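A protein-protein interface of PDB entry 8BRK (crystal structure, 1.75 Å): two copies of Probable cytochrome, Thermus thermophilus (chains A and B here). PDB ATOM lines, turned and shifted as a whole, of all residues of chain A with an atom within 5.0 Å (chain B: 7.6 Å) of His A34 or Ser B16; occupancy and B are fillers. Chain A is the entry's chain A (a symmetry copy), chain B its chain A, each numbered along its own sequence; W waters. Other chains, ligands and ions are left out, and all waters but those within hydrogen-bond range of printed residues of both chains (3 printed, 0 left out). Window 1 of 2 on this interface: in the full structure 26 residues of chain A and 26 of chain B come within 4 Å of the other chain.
OH of Tyr A36 lies within hydrogen-bond range of ND1 of His B13 (2.6 Å).
N of Ser B16 is in hydrogen-bond range of OE1 of Glu A75, at 3.3 Å.
The backbone carbonyl oxygen (O) of Glu B18 is in hydrogen-bond range of the backbone NH (N) of Leu A73.
The side-chain hydroxyl (OH) of Tyr B36 sits at hydrogen-bond distance from a ring nitrogen (ND1) of His A13, 2.6 Å away.
OE1 of Glu B75 is in hydrogen-bond range of N of Ser A16.
NH2 of Arg B134 is in salt-bridge range of OE2 of Glu A75, at 2.8 Å.
OG of Ser B16 is in hydrogen-bond range of NE2 of His B13, at 2.7 Å.
NE2 of His B34 sits at hydrogen-bond distance from OE2 of Glu B75 (2.7 Å).
A ring nitrogen (NE2) of His A13 lies within hydrogen-bond range of the backbone carbonyl oxygen (O) of Lys A15.
ND1 of His A34 is in hydrogen-bond range of OG of Ser A16 (2.6 Å).
NE2 of His A34 sits at hydrogen-bond distance from OE2 of Glu A75, at 2.7 Å.
The backbone carbonyl oxygen (O) of Tyr A36 is in hydrogen-bond range of the backbone NH (N) of Val A60, 2.9 Å away.
Among the printed residues, merely in contact across the chains: Ser A16 with His B34 (3.3 Å), His A34 with Ser B16 (3.3 Å), Leu A73 with Met B17 (3.4 Å), Leu A64 with Arg B134 (3.6 Å), His A34 with His B13 (3.6 Å), His A13 with His B34 (3.6 Å), Lys A15 with Glu B75 (3.6 Å), Glu A75 with Lys B15 (3.6 Å), His A34 with Arg B134 (3.7 Å) and His A13 with His B13 (3.97 Å).
His A34 touches just these residues of chain B: His B13, Ser B16 and Arg B134.
Of the printed residues of chain B, Glu A75 touches Lys B15 (3.6 Å), Ser B16 (3.3 Å) and Arg B134 (2.8 Å).
Printed residues of chain A within 4 Å of His B13: His A13 (3.97 Å), His A34 (3.6 Å) and Tyr A36 (2.6 Å).
Printed residues of chain A within 4 Å of Ser B16: His A34 and Glu A75.
Leu B32 touches none of the printed residues of chain A.
Of the printed residues of chain A, His B34 touches His A13 and Ser A16.
Of the printed residues of chain A, Tyr B36 touches His A13.
The nearest residue of chain B that does not touch His A34 is His B34 (4.7 Å).
The nearest printed residue of chain A that does not touch Arg B134 is Tyr A36 (4.1 Å).
Of the 14 printed residues of chain A, 8 touch a printed residue of chain B.
Hydrophobic or aromatic side chains of chain A within 4 Å of the printed part of chain B: His A13, His A34, Tyr A36, Leu A64 and Leu A73.
Hydrophobic or aromatic side chains of chain B that line the printed part of chain A: His B13, Met B17, His B34 and Tyr B36.
Among the printed residues, 16 pairs touch across the chains.
Among the printed residues, Asp or Glu carboxylates within 4 Å of a Lys or Arg side-chain nitrogen of the other chain: Glu A75 with Arg B134 (2.8 Å).
His B13 touches its own counterpart, His A13.
His A13 touches His B34, and with the chains exchanged His A34 touches His B13.
His A13 touches Tyr B36, and with the chains exchanged Tyr A36 touches His B13.
Lys A15 touches Glu B75, and with the chains exchanged Glu A75 touches Lys B15.
9 positions are printed for both chains.
Of the 16 pairs that touch across the chains among the printed residues, 11 have their exchanged pair printed and touching as well.
Water W1 lies within hydrogen-bond range of the side-chain carboxylate of Asp A62, the guanidinium group of Arg B134 and the side-chain hydroxyl of Tyr A36.
Water W3 lies within hydrogen-bond range of O of Ser B16 (2.6 Å) and N of Glu A75 (2.9 Å).
Water W2 bridges the backbone carbonyl oxygen (O) of Ser A16 (2.6 Å) and the backbone NH (N) of Glu B75 (2.9 Å).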
ATOM      1  N   HIS A  13      -0.362  -5.745  18.325  1.00  0.00           N
ATOM      2  CA  HIS A  13      -1.061  -7.051  18.288  1.00  0.00           C
ATOM      3  C   HIS A  13      -1.425  -7.463  19.720  1.00  0.00           C
ATOM      4  O   HIS A  13      -0.523  -7.759  20.531  1.00  0.00           O
ATOM      5  CB  HIS A  13      -0.172  -8.059  17.551  1.00  0.00           C
ATOM      6  CG  HIS A  13      -0.725  -9.447  17.539  1.00  0.00           C
ATOM      7  ND1 HIS A  13       0.065 -10.536  17.835  1.00  0.00           N
ATOM      8  CD2 HIS A  13      -1.969  -9.914  17.314  1.00  0.00           C
ATOM      9  CE1 HIS A  13      -0.652 -11.633  17.732  1.00  0.00           C
ATOM     10  NE2 HIS A  13      -1.909 -11.283  17.435  1.00  0.00           N
ATOM     11  N   LYS A  15      -3.811 -10.028  20.712  1.00  0.00           N
ATOM     12  CA  LYS A  15      -3.996 -11.489  20.836  1.00  0.00           C
ATOM     13  C   LYS A  15      -4.526 -12.047  19.533  1.00  0.00           C
ATOM     14  O   LYS A  15      -5.011 -11.289  18.736  1.00  0.00           O
ATOM     15  CB  LYS A  15      -5.018 -11.832  21.926  1.00  0.00           C
ATOM     16  CG  LYS A  15      -6.463 -11.485  21.589  1.00  0.00           C
ATOM     17  CD  LYS A  15      -7.439 -11.936  22.647  1.00  0.00           C
ATOM     18  CE  LYS A  15      -7.617 -13.439  22.615  1.00  0.00           C
ATOM     19  NZ  LYS A  15      -8.647 -13.865  23.583  1.00  0.00           N
ATOM     20  N   SER A  16      -4.550 -13.359  19.442  1.00  0.00           N
ATOM     21  CA  SER A  16      -5.116 -14.088  18.291  1.00  0.00           C
ATOM     22  C   SER A  16      -5.961 -15.218  18.849  1.00  0.00           C
ATOM     23  O   SER A  16      -5.680 -15.705  19.963  1.00  0.00           O
ATOM     24  CB  SER A  16      -4.038 -14.608  17.403  1.00  0.00           C
ATOM     25  OG  SER A  16      -3.264 -13.539  16.899  1.00  0.00           O
ATOM     26  N   LEU A  32      -9.846 -17.227  11.852  1.00  0.00           N
ATOM     27  CA  LEU A  32      -8.718 -16.791  12.698  1.00  0.00           C
ATOM     28  C   LEU A  32      -8.853 -15.282  12.840  1.00  0.00           C
ATOM     29  O   LEU A  32      -8.882 -14.610  11.817  1.00  0.00           O
ATOM     30  CB  LEU A  32      -7.392 -17.159  12.031  1.00  0.00           C
ATOM     31  CG  LEU A  32      -6.149 -16.678  12.770  1.00  0.00           C
ATOM     32  CD1 LEU A  32      -6.041 -17.332  14.141  1.00  0.00           C
ATOM     33  CD2 LEU A  32      -4.918 -16.984  11.954  1.00  0.00           C
ATOM     34  N   HIS A  33      -8.928 -14.778  14.059  1.00  0.00           N
ATOM     35  CA  HIS A  33      -8.923 -13.317  14.241  1.00  0.00           C
ATOM     36  C   HIS A  33      -7.700 -12.861  15.028  1.00  0.00           C
ATOM     37  O   HIS A  33      -7.174 -13.568  15.901  1.00  0.00           O
ATOM     38  CB  HIS A  33     -10.242 -12.825  14.819  1.00  0.00           C
ATOM     39  CG  HIS A  33     -10.476 -13.175  16.254  1.00  0.00           C
ATOM     40  ND1 HIS A  33     -11.321 -14.213  16.628  1.00  0.00           N
ATOM     41  CD2 HIS A  33     -10.061 -12.574  17.386  1.00  0.00           C
ATOM     42  CE1 HIS A  33     -11.437 -14.232  17.937  1.00  0.00           C
ATOM     43  NE2 HIS A  33     -10.646 -13.238  18.433  1.00  0.00           N
ATOM     44  N   HIS A  34      -7.309 -11.644  14.728  1.00  0.00           N
ATOM     45  CA  HIS A  34      -6.250 -10.921  15.452  1.00  0.00           C
ATOM     46  C   HIS A  34      -6.876  -9.640  15.945  1.00  0.00           C
ATOM     47  O   HIS A  34      -7.619  -8.999  15.166  1.00  0.00           O
ATOM     48  CB  HIS A  34      -5.090 -10.589  14.517  1.00  0.00           C
ATOM     49  CG  HIS A  34      -4.542 -11.766  13.804  1.00  0.00           C
ATOM     50  ND1 HIS A  34      -3.830 -12.734  14.466  1.00  0.00           N
ATOM     51  CD2 HIS A  34      -4.567 -12.115  12.498  1.00  0.00           C
ATOM     52  CE1 HIS A  34      -3.431 -13.636  13.583  1.00  0.00           C
ATOM     53  NE2 HIS A  34      -3.859 -13.282  12.386  1.00  0.00           N
ATOM     54  N   ILE A  35      -6.516  -9.252  17.150  1.00  0.00           N
ATOM     55  CA  ILE A  35      -6.959  -7.970  17.724  1.00  0.00           C
ATOM     56  C   ILE A  35      -5.758  -7.012  17.773  1.00  0.00           C
ATOM     57  O   ILE A  35      -4.643  -7.426  18.169  1.00  0.00           O
ATOM     58  CB  ILE A  35      -7.653  -8.233  19.065  1.00  0.00           C
ATOM     59  CG1 ILE A  35      -8.938  -9.042  18.842  1.00  0.00           C
ATOM     60  CG2 ILE A  35      -7.933  -6.935  19.790  1.00  0.00           C
ATOM     61  CD1 ILE A  35      -9.507  -9.634  20.088  1.00  0.00           C
ATOM     62  N   TYR A  36      -6.006  -5.779  17.364  1.00  0.00           N
ATOM     63  CA  TYR A  36      -5.025  -4.678  17.358  1.00  0.00           C
ATOM     64  C   TYR A  36      -5.599  -3.507  18.154  1.00  0.00           C
ATOM     65  O   TYR A  36      -6.792  -3.223  18.080  1.00  0.00           O
ATOM     66  CB  TYR A  36      -4.671  -4.271  15.927  1.00  0.00           C
ATOM     67  CG  TYR A  36      -4.102  -5.380  15.091  1.00  0.00           C
ATOM     68  CD1 TYR A  36      -2.751  -5.672  15.091  1.00  0.00           C
ATOM     69  CD2 TYR A  36      -4.933  -6.149  14.294  1.00  0.00           C
ATOM     70  CE1 TYR A  36      -2.257  -6.744  14.363  1.00  0.00           C
ATOM     71  CE2 TYR A  36      -4.446  -7.189  13.529  1.00  0.00           C
ATOM     72  CZ  TYR A  36      -3.105  -7.496  13.573  1.00  0.00           C
ATOM     73  OH  TYR A  36      -2.650  -8.553  12.844  1.00  0.00           O
ATOM     74  N   VAL A  60      -9.344  -2.995  16.809  1.00  0.00           N
ATOM     75  CA  VAL A  60      -9.697  -3.664  15.529  1.00  0.00           C
ATOM     76  C   VAL A  60      -9.671  -5.164  15.756  1.00  0.00           C
ATOM     77  O   VAL A  60      -8.688  -5.691  16.340  1.00  0.00           O
ATOM     78  CB  VAL A  60      -8.797  -3.214  14.373  1.00  0.00           C
ATOM     79  CG1 VAL A  60      -9.089  -3.968  13.098  1.00  0.00           C
ATOM     80  CG2 VAL A  60      -8.973  -1.719  14.144  1.00  0.00           C
ATOM     81  N   PHE A  61     -10.775  -5.777  15.349  1.00  0.00           N
ATOM     82  CA  PHE A  61     -10.962  -7.232  15.247  1.00  0.00           C
ATOM     83  C   PHE A  61     -10.789  -7.581  13.778  1.00  0.00           C
ATOM     84  O   PHE A  61     -11.646  -7.191  12.950  1.00  0.00           O
ATOM     85  CB  PHE A  61     -12.355  -7.554  15.785  1.00  0.00           C
ATOM     86  CG  PHE A  61     -12.714  -9.014  15.839  1.00  0.00           C
ATOM     87  CD1 PHE A  61     -13.131  -9.676  14.696  1.00  0.00           C
ATOM     88  CD2 PHE A  61     -12.715  -9.691  17.046  1.00  0.00           C
ATOM     89  CE1 PHE A  61     -13.527 -10.998  14.761  1.00  0.00           C
ATOM     90  CE2 PHE A  61     -13.127 -11.008  17.100  1.00  0.00           C
ATOM     91  CZ  PHE A  61     -13.493 -11.663  15.952  1.00  0.00           C
ATOM     92  N   ASP A  62      -9.671  -8.225  13.465  1.00  0.00           N
ATOM     93  CA  ASP A  62      -9.285  -8.555  12.081  1.00  0.00           C
ATOM     94  C   ASP A  62      -9.597 -10.025  11.864  1.00  0.00           C
ATOM     95  O   ASP A  62      -8.904 -10.858  12.447  1.00  0.00           O
ATOM     96  CB  ASP A  62      -7.827  -8.235  11.815  1.00  0.00           C
ATOM     97  CG  ASP A  62      -7.497  -8.154  10.333  1.00  0.00           C
ATOM     98  OD1 ASP A  62      -8.339  -8.592   9.477  1.00  0.00           O
ATOM     99  OD2 ASP A  62      -6.395  -7.690  10.037  1.00  0.00           O
ATOM    100  N   LEU A  64      -9.844 -13.351   9.495  1.00  0.00           N
ATOM    101  CA  LEU A  64      -9.322 -14.023   8.287  1.00  0.00           C
ATOM    102  C   LEU A  64      -9.939 -15.411   8.224  1.00  0.00           C
ATOM    103  O   LEU A  64     -10.183 -15.967   9.284  1.00  0.00           O
ATOM    104  CB  LEU A  64      -7.797 -14.121   8.396  1.00  0.00           C
ATOM    105  CG  LEU A  64      -7.077 -12.821   8.736  1.00  0.00           C
ATOM    106  CD1 LEU A  64      -5.597 -13.067   8.938  1.00  0.00           C
ATOM    107  CD2 LEU A  64      -7.291 -11.813   7.637  1.00  0.00           C
ATOM    108  N   LEU A  73      -2.028 -24.494  10.015  1.00  0.00           N
ATOM    109  CA  LEU A  73      -3.090 -23.469   9.882  1.00  0.00           C
ATOM    110  C   LEU A  73      -2.449 -22.220   9.287  1.00  0.00           C
ATOM    111  O   LEU A  73      -1.499 -21.673   9.874  1.00  0.00           O
ATOM    112  CB  LEU A  73      -3.705 -23.187  11.255  1.00  0.00           C
ATOM    113  CG  LEU A  73      -4.689 -22.008  11.323  1.00  0.00           C
ATOM    114  CD1 LEU A  73      -5.886 -22.214  10.444  1.00  0.00           C
ATOM    115  CD2 LEU A  73      -5.153 -21.785  12.748  1.00  0.00           C
ATOM    116  N   GLU A  75      -3.168 -18.310   7.361  1.00  0.00           N
ATOM    117  CA  GLU A  75      -4.079 -17.163   7.171  1.00  0.00           C
ATOM    118  C   GLU A  75      -4.642 -17.163   5.751  1.00  0.00           C
ATOM    119  O   GLU A  75      -3.895 -17.097   4.824  1.00  0.00           O
ATOM    120  CB  GLU A  75      -3.314 -15.894   7.497  1.00  0.00           C
ATOM    121  CG  GLU A  75      -2.748 -15.960   8.902  1.00  0.00           C
ATOM    122  CD  GLU A  75      -2.014 -14.698   9.258  1.00  0.00           C
ATOM    123  OE1 GLU A  75      -1.102 -14.343   8.484  1.00  0.00           O
ATOM    124  OE2 GLU A  75      -2.435 -14.048  10.236  1.00  0.00           O
ATOM    125  N   HIS B  13       3.134  -6.748  13.459  1.00  0.00           N
ATOM    126  CA  HIS B  13       2.733  -8.161  13.268  1.00  0.00           C
ATOM    127  C   HIS B  13       2.794  -8.498  11.772  1.00  0.00           C
ATOM    128  O   HIS B  13       1.987  -7.968  10.981  1.00  0.00           O
ATOM    129  CB  HIS B  13       1.354  -8.368  13.902  1.00  0.00           C
ATOM    130  CG  HIS B  13       0.793  -9.735  13.682  1.00  0.00           C
ATOM    131  ND1 HIS B  13      -0.512  -9.919  13.278  1.00  0.00           N
ATOM    132  CD2 HIS B  13       1.354 -10.957  13.764  1.00  0.00           C
ATOM    133  CE1 HIS B  13      -0.759 -11.206  13.180  1.00  0.00           C
ATOM    134  NE2 HIS B  13       0.372 -11.869  13.450  1.00  0.00           N
ATOM    135  N   VAL B  14       3.691  -9.389  11.384  1.00  0.00           N
ATOM    136  CA  VAL B  14       3.935  -9.698   9.945  1.00  0.00           C
ATOM    137  C   VAL B  14       2.933 -10.759   9.496  1.00  0.00           C
ATOM    138  O   VAL B  14       2.291 -10.589   8.454  1.00  0.00           O
ATOM    139  CB  VAL B  14       5.389 -10.146   9.762  1.00  0.00           C
ATOM    140  CG1 VAL B  14       5.666 -10.693   8.355  1.00  0.00           C
ATOM    141  CG2 VAL B  14       6.313  -9.019  10.129  1.00  0.00           C
ATOM    142  N   LYS B  15       2.801 -11.821  10.284  1.00  0.00           N
ATOM    143  CA  LYS B  15       1.932 -12.966   9.939  1.00  0.00           C
ATOM    144  C   LYS B  15       1.852 -13.915  11.116  1.00  0.00           C
ATOM    145  O   LYS B  15       2.680 -13.828  11.984  1.00  0.00           O
ATOM    146  CB  LYS B  15       2.495 -13.758   8.754  1.00  0.00           C
ATOM    147  CG  LYS B  15       3.756 -14.558   9.052  1.00  0.00           C
ATOM    148  CD  LYS B  15       4.210 -15.400   7.886  1.00  0.00           C
ATOM    149  CE  LYS B  15       3.299 -16.592   7.690  1.00  0.00           C
ATOM    150  NZ  LYS B  15       3.803 -17.467   6.613  1.00  0.00           N
ATOM    151  N   SER B  16       0.959 -14.875  11.015  1.00  0.00           N
ATOM    152  CA  SER B  16       0.796 -15.948  12.014  1.00  0.00           C
ATOM    153  C   SER B  16       0.657 -17.253  11.250  1.00  0.00           C
ATOM    154  O   SER B  16       0.183 -17.243  10.096  1.00  0.00           O
ATOM    155  CB  SER B  16      -0.392 -15.700  12.879  1.00  0.00           C
ATOM    156  OG  SER B  16      -0.241 -14.481  13.576  1.00  0.00           O
ATOM    157  N   MET B  17       1.018 -18.339  11.901  1.00  0.00           N
ATOM    158  CA  MET B  17       0.876 -19.686  11.327  1.00  0.00           C
ATOM    159  C   MET B  17       0.921 -20.687  12.479  1.00  0.00           C
ATOM    160  O   MET B  17       1.718 -20.496  13.408  1.00  0.00           O
ATOM    161  CB  MET B  17       2.045 -19.916  10.382  1.00  0.00           C
ATOM    162  CG  MET B  17       1.934 -21.127   9.541  1.00  0.00           C
ATOM    163  SD  MET B  17       3.412 -21.227   8.513  1.00  0.00           S
ATOM    164  CE  MET B  17       2.931 -22.588   7.460  1.00  0.00           C
ATOM    165  N   GLU B  18       0.124 -21.746  12.382  1.00  0.00           N
ATOM    166  CA  GLU B  18       0.165 -22.852  13.361  1.00  0.00           C
ATOM    167  C   GLU B  18       0.753 -24.057  12.644  1.00  0.00           C
ATOM    168  O   GLU B  18       0.308 -24.355  11.557  1.00  0.00           O
ATOM    169  CB  GLU B  18      -1.193 -23.161  13.976  1.00  0.00           C
ATOM    170  CG  GLU B  18      -1.087 -24.184  15.095  1.00  0.00           C
ATOM    171  CD  GLU B  18      -2.239 -25.158  15.198  1.00  0.00           C
ATOM    172  OE1 GLU B  18      -3.168 -25.055  14.377  1.00  0.00           O
ATOM    173  OE2 GLU B  18      -2.196 -25.994  16.113  1.00  0.00           O
ATOM    174  N   LEU B  32       1.662 -22.368  17.646  1.00  0.00           N
ATOM    175  CA  LEU B  32       1.199 -21.157  16.940  1.00  0.00           C
ATOM    176  C   LEU B  32       2.347 -20.161  17.008  1.00  0.00           C
ATOM    177  O   LEU B  32       2.773 -19.852  18.114  1.00  0.00           O
ATOM    178  CB  LEU B  32      -0.050 -20.599  17.622  1.00  0.00           C
ATOM    179  CG  LEU B  32      -0.570 -19.293  17.034  1.00  0.00           C
ATOM    180  CD1 LEU B  32      -1.020 -19.484  15.592  1.00  0.00           C
ATOM    181  CD2 LEU B  32      -1.716 -18.777  17.868  1.00  0.00           C
ATOM    182  N   HIS B  33       2.820 -19.680  15.873  1.00  0.00           N
ATOM    183  CA  HIS B  33       3.836 -18.615  15.904  1.00  0.00           C
ATOM    184  C   HIS B  33       3.315 -17.334  15.264  1.00  0.00           C
ATOM    185  O   HIS B  33       2.499 -17.346  14.330  1.00  0.00           O
ATOM    186  CB  HIS B  33       5.161 -19.094  15.327  1.00  0.00           C
ATOM    187  CG  HIS B  33       5.171 -19.298  13.846  1.00  0.00           C
ATOM    188  ND1 HIS B  33       5.085 -20.562  13.278  1.00  0.00           N
ATOM    189  CD2 HIS B  33       5.352 -18.421  12.838  1.00  0.00           C
ATOM    190  CE1 HIS B  33       5.232 -20.467  11.975  1.00  0.00           C
ATOM    191  NE2 HIS B  33       5.377 -19.145  11.674  1.00  0.00           N
ATOM    192  N   HIS B  34       3.857 -16.245  15.758  1.00  0.00           N
ATOM    193  CA  HIS B  34       3.635 -14.897  15.209  1.00  0.00           C
ATOM    194  C   HIS B  34       5.000 -14.350  14.870  1.00  0.00           C
ATOM    195  O   HIS B  34       5.933 -14.521  15.689  1.00  0.00           O
ATOM    196  CB  HIS B  34       2.974 -13.994  16.248  1.00  0.00           C
ATOM    197  CG  HIS B  34       1.724 -14.553  16.814  1.00  0.00           C
ATOM    198  ND1 HIS B  34       0.581 -14.652  16.062  1.00  0.00           N
ATOM    199  CD2 HIS B  34       1.425 -15.006  18.053  1.00  0.00           C
ATOM    200  CE1 HIS B  34      -0.381 -15.143  16.828  1.00  0.00           C
ATOM    201  NE2 HIS B  34       0.102 -15.360  18.037  1.00  0.00           N
ATOM    202  N   ILE B  35       5.078 -13.652  13.756  1.00  0.00           N
ATOM    203  CA  ILE B  35       6.317 -12.968  13.349  1.00  0.00           C
ATOM    204  C   ILE B  35       6.115 -11.452  13.508  1.00  0.00           C
ATOM    205  O   ILE B  35       5.049 -10.918  13.122  1.00  0.00           O
ATOM    206  CB  ILE B  35       6.713 -13.440  11.945  1.00  0.00           C
ATOM    207  CG1 ILE B  35       7.068 -14.933  11.974  1.00  0.00           C
ATOM    208  CG2 ILE B  35       7.854 -12.609  11.400  1.00  0.00           C
ATOM    209  CD1 ILE B  35       7.141 -15.566  10.625  1.00  0.00           C
ATOM    210  N   TYR B  36       7.122 -10.809  14.075  1.00  0.00           N
ATOM    211  CA  TYR B  36       7.175  -9.352  14.297  1.00  0.00           C
ATOM    212  C   TYR B  36       8.445  -8.804  13.646  1.00  0.00           C
ATOM    213  O   TYR B  36       9.496  -9.437  13.690  1.00  0.00           O
ATOM    214  CB  TYR B  36       7.118  -9.025  15.790  1.00  0.00           C
ATOM    215  CG  TYR B  36       5.892  -9.538  16.489  1.00  0.00           C
ATOM    216  CD1 TYR B  36       4.717  -8.812  16.525  1.00  0.00           C
ATOM    217  CD2 TYR B  36       5.915 -10.772  17.117  1.00  0.00           C
ATOM    218  CE1 TYR B  36       3.578  -9.335  17.120  1.00  0.00           C
ATOM    219  CE2 TYR B  36       4.801 -11.283  17.752  1.00  0.00           C
ATOM    220  CZ  TYR B  36       3.625 -10.568  17.741  1.00  0.00           C
ATOM    221  OH  TYR B  36       2.524 -11.108  18.336  1.00  0.00           O
ATOM    222  N   GLU B  75      -4.161 -19.170  22.316  1.00  0.00           N
ATOM    223  CA  GLU B  75      -2.724 -19.014  22.616  1.00  0.00           C
ATOM    224  C   GLU B  75      -2.401 -19.608  23.986  1.00  0.00           C
ATOM    225  O   GLU B  75      -2.947 -19.178  24.955  1.00  0.00           O
ATOM    226  CB  GLU B  75      -2.379 -17.539  22.522  1.00  0.00           C
ATOM    227  CG  GLU B  75      -2.751 -16.992  21.157  1.00  0.00           C
ATOM    228  CD  GLU B  75      -2.388 -15.540  21.030  1.00  0.00           C
ATOM    229  OE1 GLU B  75      -2.845 -14.769  21.899  1.00  0.00           O
ATOM    230  OE2 GLU B  75      -1.578 -15.229  20.133  1.00  0.00           O
ATOM    231  N   ALA B 132       6.313 -13.692   4.360  1.00  0.00           N
ATOM    232  CA  ALA B 132       5.876 -12.494   3.617  1.00  0.00           C
ATOM    233  C   ALA B 132       4.890 -11.739   4.506  1.00  0.00           C
ATOM    234  O   ALA B 132       4.190 -12.357   5.335  1.00  0.00           O
ATOM    235  CB  ALA B 132       5.266 -12.883   2.291  1.00  0.00           C
ATOM    236  N   ARG B 134       1.570 -10.149   5.427  1.00  0.00           N
ATOM    237  CA  ARG B 134       0.188 -10.505   5.041  1.00  0.00           C
ATOM    238  C   ARG B 134      -0.612  -9.232   5.265  1.00  0.00           C
ATOM    239  O   ARG B 134      -0.752  -8.800   6.407  1.00  0.00           O
ATOM    240  CB  ARG B 134      -0.274 -11.693   5.892  1.00  0.00           C
ATOM    241  CG  ARG B 134      -1.594 -12.315   5.428  1.00  0.00           C
ATOM    242  CD  ARG B 134      -2.769 -11.803   6.210  1.00  0.00           C
ATOM    243  NE  ARG B 134      -2.419 -11.909   7.608  1.00  0.00           N
ATOM    244  CZ  ARG B 134      -2.685 -11.015   8.548  1.00  0.00           C
ATOM    245  NH1 ARG B 134      -3.335  -9.903   8.257  1.00  0.00           N
ATOM    246  NH2 ARG B 134      -2.285 -11.242   9.785  1.00  0.00           N
HETATM  247  O   HOH W   1      -4.108  -8.842  10.555  1.00  0.00           O
HETATM  248  O   HOH W   2      -6.091 -17.031  22.206  1.00  0.00           O
HETATM  249  O   HOH W   3      -0.306 -18.143   7.666  1.00  0.00           O
